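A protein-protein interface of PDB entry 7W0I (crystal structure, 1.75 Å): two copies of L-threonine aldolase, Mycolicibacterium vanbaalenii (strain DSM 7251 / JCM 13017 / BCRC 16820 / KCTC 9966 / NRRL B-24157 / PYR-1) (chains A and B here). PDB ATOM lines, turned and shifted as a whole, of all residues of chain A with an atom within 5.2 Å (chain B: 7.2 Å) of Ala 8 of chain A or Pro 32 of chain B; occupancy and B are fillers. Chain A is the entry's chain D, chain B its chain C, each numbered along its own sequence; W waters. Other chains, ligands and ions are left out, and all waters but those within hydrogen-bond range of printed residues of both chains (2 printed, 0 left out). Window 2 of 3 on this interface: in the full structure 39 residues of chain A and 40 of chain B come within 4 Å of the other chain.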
ATOM      1  N   SER A   6      29.456  11.969 -13.044  1.00  0.00           N
ATOM      2  CA  SER A   6      28.934  10.602 -13.001  1.00  0.00           C
ATOM      3  C   SER A   6      30.038   9.590 -12.741  1.00  0.00           C
ATOM      4  O   SER A   6      31.095   9.651 -13.367  1.00  0.00           O
ATOM      5  CB  SER A   6      28.231  10.260 -14.316  1.00  0.00           C
ATOM      6  OG  SER A   6      27.917   8.878 -14.387  1.00  0.00           O
ATOM      7  N   ALA A   7      29.771   8.635 -11.846  1.00  0.00           N
ATOM      8  CA  ALA A   7      30.717   7.581 -11.506  1.00  0.00           C
ATOM      9  C   ALA A   7      30.487   6.291 -12.293  1.00  0.00           C
ATOM     10  O   ALA A   7      31.060   5.253 -11.942  1.00  0.00           O
ATOM     11  CB  ALA A   7      30.656   7.294 -10.003  1.00  0.00           C
ATOM     12  N   ALA A   8      29.694   6.341 -13.370  1.00  0.00           N
ATOM     13  CA  ALA A   8      29.325   5.122 -14.090  1.00  0.00           C
ATOM     14  C   ALA A   8      30.541   4.356 -14.605  1.00  0.00           C
ATOM     15  O   ALA A   8      30.485   3.128 -14.732  1.00  0.00           O
ATOM     16  CB  ALA A   8      28.397   5.459 -15.257  1.00  0.00           C
ATOM     17  N   PHE A   9      31.646   5.048 -14.893  1.00  0.00           N
ATOM     18  CA  PHE A   9      32.838   4.405 -15.433  1.00  0.00           C
ATOM     19  C   PHE A   9      34.065   4.632 -14.565  1.00  0.00           C
ATOM     20  O   PHE A   9      35.179   4.329 -15.002  1.00  0.00           O
ATOM     21  CB  PHE A   9      33.097   4.894 -16.864  1.00  0.00           C
ATOM     22  CG  PHE A   9      31.976   4.566 -17.815  1.00  0.00           C
ATOM     23  CD1 PHE A   9      31.837   3.286 -18.320  1.00  0.00           C
ATOM     24  CD2 PHE A   9      31.036   5.529 -18.165  1.00  0.00           C
ATOM     25  CE1 PHE A   9      30.785   2.967 -19.179  1.00  0.00           C
ATOM     26  CE2 PHE A   9      29.984   5.224 -19.021  1.00  0.00           C
ATOM     27  CZ  PHE A   9      29.858   3.938 -19.532  1.00  0.00           C
ATOM     28  N   ALA A  10      33.890   5.156 -13.349  1.00  0.00           N
ATOM     29  CA  ALA A  10      35.039   5.424 -12.494  1.00  0.00           C
ATOM     30  C   ALA A  10      35.774   4.139 -12.142  1.00  0.00           C
ATOM     31  O   ALA A  10      37.008   4.084 -12.200  1.00  0.00           O
ATOM     32  CB  ALA A  10      34.591   6.155 -11.229  1.00  0.00           C
ATOM     33  N   SER A  11      35.029   3.091 -11.815  1.00  0.00           N
ATOM     34  CA  SER A  11      35.585   1.791 -11.473  1.00  0.00           C
ATOM     35  C   SER A  11      34.422   0.813 -11.401  1.00  0.00           C
ATOM     36  O   SER A  11      33.268   1.219 -11.237  1.00  0.00           O
ATOM     37  CB  SER A  11      36.340   1.830 -10.138  1.00  0.00           C
ATOM     38  OG  SER A  11      36.663   0.518  -9.705  1.00  0.00           O
ATOM     39  N   ALA A  14      32.618   1.215  -8.210  1.00  0.00           N
ATOM     40  CA  ALA A  14      31.629   2.274  -8.086  1.00  0.00           C
ATOM     41  C   ALA A  14      30.207   1.750  -8.222  1.00  0.00           C
ATOM     42  O   ALA A  14      29.255   2.480  -7.912  1.00  0.00           O
ATOM     43  CB  ALA A  14      31.882   3.362  -9.131  1.00  0.00           C
ATOM     44  N   ALA A  15      30.043   0.512  -8.671  1.00  0.00           N
ATOM     45  CA  ALA A  15      28.729  -0.058  -8.905  1.00  0.00           C
ATOM     46  C   ALA A  15      28.059  -0.421  -7.585  1.00  0.00           C
ATOM     47  O   ALA A  15      28.732  -0.643  -6.574  1.00  0.00           O
ATOM     48  CB  ALA A  15      28.848  -1.290  -9.802  1.00  0.00           C
ATOM     49  N   PRO A  16      26.713  -0.467  -7.559  1.00  0.00           N
ATOM     50  CA  PRO A  16      26.018  -0.943  -6.355  1.00  0.00           C
ATOM     51  C   PRO A  16      26.141  -2.455  -6.223  1.00  0.00           C
ATOM     52  O   PRO A  16      26.931  -3.077  -6.938  1.00  0.00           O
ATOM     53  CB  PRO A  16      24.566  -0.500  -6.588  1.00  0.00           C
ATOM     54  CG  PRO A  16      24.417  -0.526  -8.072  1.00  0.00           C
ATOM     55  CD  PRO A  16      25.773  -0.166  -8.659  1.00  0.00           C
ATOM     56  N   TYR A 306      32.156  12.872 -16.759  1.00  0.00           N
ATOM     57  CA  TYR A 306      32.374  11.496 -16.323  1.00  0.00           C
ATOM     58  C   TYR A 306      33.623  11.447 -15.466  1.00  0.00           C
ATOM     59  O   TYR A 306      34.644  12.047 -15.813  1.00  0.00           O
ATOM     60  CB  TYR A 306      32.516  10.511 -17.489  1.00  0.00           C
ATOM     61  CG  TYR A 306      31.192  10.168 -18.088  1.00  0.00           C
ATOM     62  CD1 TYR A 306      30.359   9.236 -17.489  1.00  0.00           C
ATOM     63  CD2 TYR A 306      30.741  10.824 -19.220  1.00  0.00           C
ATOM     64  CE1 TYR A 306      29.125   8.941 -18.028  1.00  0.00           C
ATOM     65  CE2 TYR A 306      29.512  10.545 -19.766  1.00  0.00           C
ATOM     66  CZ  TYR A 306      28.704   9.602 -19.168  1.00  0.00           C
ATOM     67  OH  TYR A 306      27.471   9.314 -19.711  1.00  0.00           O
ATOM     68  N   VAL A 321      35.960   1.934 -16.728  1.00  0.00           N
ATOM     69  CA  VAL A 321      35.715   0.575 -16.264  1.00  0.00           C
ATOM     70  C   VAL A 321      34.220   0.310 -16.317  1.00  0.00           C
ATOM     71  O   VAL A 321      33.423   1.118 -15.823  1.00  0.00           O
ATOM     72  CB  VAL A 321      36.259   0.333 -14.847  1.00  0.00           C
ATOM     73  CG1 VAL A 321      36.190  -1.150 -14.524  1.00  0.00           C
ATOM     74  CG2 VAL A 321      37.695   0.859 -14.727  1.00  0.00           C
ATOM     75  N   THR A 326      26.457  -1.698 -15.642  1.00  0.00           N
ATOM     76  CA  THR A 326      26.566  -0.758 -16.752  1.00  0.00           C
ATOM     77  C   THR A 326      25.519  -1.071 -17.818  1.00  0.00           C
ATOM     78  O   THR A 326      25.286  -2.233 -18.165  1.00  0.00           O
ATOM     79  CB  THR A 326      27.975  -0.797 -17.360  1.00  0.00           C
ATOM     80  OG1 THR A 326      28.944  -0.498 -16.344  1.00  0.00           O
ATOM     81  CG2 THR A 326      28.098   0.236 -18.462  1.00  0.00           C
ATOM     82  N   GLU A 330      24.352   4.102 -20.926  1.00  0.00           N
ATOM     83  CA  GLU A 330      25.491   4.790 -20.325  1.00  0.00           C
ATOM     84  C   GLU A 330      26.684   4.805 -21.272  1.00  0.00           C
ATOM     85  O   GLU A 330      27.357   5.835 -21.429  1.00  0.00           O
ATOM     86  CB  GLU A 330      25.868   4.115 -19.003  1.00  0.00           C
ATOM     87  CG  GLU A 330      24.868   4.331 -17.871  1.00  0.00           C
ATOM     88  CD  GLU A 330      25.216   3.530 -16.625  1.00  0.00           C
ATOM     89  OE1 GLU A 330      25.874   2.476 -16.758  1.00  0.00           O
ATOM     90  OE2 GLU A 330      24.839   3.965 -15.512  1.00  0.00           O
ATOM     91  N   GLN B  30      21.487   2.039  -5.071  1.00  0.00           N
ATOM     92  CA  GLN B  30      21.104   2.311  -6.454  1.00  0.00           C
ATOM     93  C   GLN B  30      22.076   3.281  -7.107  1.00  0.00           C
ATOM     94  O   GLN B  30      22.546   4.233  -6.475  1.00  0.00           O
ATOM     95  CB  GLN B  30      19.678   2.863  -6.572  1.00  0.00           C
ATOM     96  CG  GLN B  30      19.353   4.030  -5.667  1.00  0.00           C
ATOM     97  CD  GLN B  30      18.407   3.624  -4.559  1.00  0.00           C
ATOM     98  OE1 GLN B  30      18.329   2.449  -4.197  1.00  0.00           O
ATOM     99  NE2 GLN B  30      17.656   4.588  -4.034  1.00  0.00           N
ATOM    100  N   GLY B  31      22.383   3.019  -8.374  1.00  0.00           N
ATOM    101  CA  GLY B  31      23.213   3.891  -9.163  1.00  0.00           C
ATOM    102  C   GLY B  31      24.670   3.763  -8.777  1.00  0.00           C
ATOM    103  O   GLY B  31      25.009   3.154  -7.758  1.00  0.00           O
ATOM    104  N   PRO B  32      25.561   4.305  -9.599  1.00  0.00           N
ATOM    105  CA  PRO B  32      26.976   4.342  -9.227  1.00  0.00           C
ATOM    106  C   PRO B  32      27.243   5.441  -8.211  1.00  0.00           C
ATOM    107  O   PRO B  32      26.521   6.436  -8.127  1.00  0.00           O
ATOM    108  CB  PRO B  32      27.694   4.625 -10.550  1.00  0.00           C
ATOM    109  CG  PRO B  32      26.665   5.268 -11.420  1.00  0.00           C
ATOM    110  CD  PRO B  32      25.325   4.765 -10.978  1.00  0.00           C
ATOM    111  N   ALA B  33      28.315   5.250  -7.439  1.00  0.00           N
ATOM    112  CA  ALA B  33      28.723   6.204  -6.420  1.00  0.00           C
ATOM    113  C   ALA B  33      30.243   6.276  -6.364  1.00  0.00           C
ATOM    114  O   ALA B  33      30.913   5.234  -6.440  1.00  0.00           O
ATOM    115  CB  ALA B  33      28.168   5.828  -5.037  1.00  0.00           C
ATOM    116  N   PRO B  34      30.813   7.477  -6.236  1.00  0.00           N
ATOM    117  CA  PRO B  34      32.274   7.590  -6.109  1.00  0.00           C
ATOM    118  C   PRO B  34      32.755   6.821  -4.890  1.00  0.00           C
ATOM    119  O   PRO B  34      32.092   6.789  -3.856  1.00  0.00           O
ATOM    120  CB  PRO B  34      32.508   9.100  -5.960  1.00  0.00           C
ATOM    121  CG  PRO B  34      31.228   9.740  -6.426  1.00  0.00           C
ATOM    122  CD  PRO B  34      30.141   8.776  -6.079  1.00  0.00           C
ATOM    123  N   ARG B 241      29.835   3.570   0.784  1.00  0.00           N
ATOM    124  CA  ARG B 241      28.457   3.909   1.107  1.00  0.00           C
ATOM    125  C   ARG B 241      27.813   2.837   1.975  1.00  0.00           C
ATOM    126  O   ARG B 241      26.963   3.156   2.802  1.00  0.00           O
ATOM    127  CB  ARG B 241      27.640   4.134  -0.163  1.00  0.00           C
ATOM    128  CG  ARG B 241      27.521   2.919  -1.067  1.00  0.00           C
ATOM    129  CD  ARG B 241      26.504   3.161  -2.184  1.00  0.00           C
ATOM    130  NE  ARG B 241      26.994   2.680  -3.474  1.00  0.00           N
ATOM    131  CZ  ARG B 241      26.354   2.798  -4.637  1.00  0.00           C
ATOM    132  NH1 ARG B 241      25.159   3.369  -4.705  1.00  0.00           N
ATOM    133  NH2 ARG B 241      26.912   2.326  -5.747  1.00  0.00           N
HETATM  134  O   HOH W   1      29.453   1.468  -4.637  1.00  0.00           O
HETATM  135  O   HOH W   2      27.503   8.933 -10.124  1.00  0.00           O
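Ala 8 of chain A touches just one residue of chain B: Pro 32 (3.8 Å). Ala 10 of chain A touches none of the printed residues of chain B. Of the printed residues of chain B, Ala 15 of chain A touches Arg 241 (3.5 Å). Printed residues of chain B within 4 Å of Pro 16 of chain A: Gly 31 (3.5 Å) and Arg 241 (3.3 Å). Of the printed residues of chain A, Gly 31 of chain B touches Pro 16. Of chain A, only Ala 7, Ala 8 and Ala 14 come within 4 Å of Pro 32 of chain B. Printed residues of chain A within 4 Å of Pro 34 of chain B: Ala 7. The nearest residue of chain A that does not touch Pro 32 of chain B is Pro 16 of chain A (4.6 Å).
Hydrophobic or aromatic side chains of chain A that line the printed part of chain B: Ala 7, Ala 14 and Pro 16.
O of Ala 14 of chain A lies within hydrogen-bond range of NH2 of Arg 241 of chain B. N of Pro 16 of chain A lies close to NH2 of Arg 241 of chain B. The backbone NH of Ala 33 of chain B lies within hydrogen-bond range of the backbone carbonyl oxygen of Ala 14 of chain A.
Among the printed residues, merely in contact across the chains: Ala 7 of chain A with Pro 32 of chain B, Ala 7 of chain A with Ala 33 of chain B, Ala 7 of chain A with Pro 34 of chain B, Ala 8 of chain A with Pro 32 of chain B, Ala 14 of chain A with Pro 32 of chain B, Ala 15 of chain A with Arg 241 of chain B and Pro 16 of chain A with Gly 31 of chain B.
No position is printed for both chains. Of the 10 pairs that touch across the chains among the printed residues, none has its exchanged pair printed and touching as well.
Water W2 lies within hydrogen-bond range of the backbone NH (N) of Ala 7 of chain A (2.9 Å) and the backbone carbonyl oxygen (O) of Pro 32 of chain B (3.3 Å). Water W1 lies within hydrogen-bond range of NH2 of Arg 241 of chain B (2.9 Å), O of Ala 15 of chain A (3.0 Å) and O of Ala 14 of chain A (3.4 Å).
The backbone carbonyl oxygen (O) of Gln 30 of chain B sits at hydrogen-bond distance from the guanidinium group (NH1) of Arg 241 of chain B, at 3.3 Å. The backbone NH (N) of Ala 8 of chain A is in hydrogen-bond range of the side-chain hydroxyl (OG) of Ser 6 of chain A. NH2 of Arg 241 of chain B is in hydrogen-bond range of O of Gly 31 of chain B (2.9 Å).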
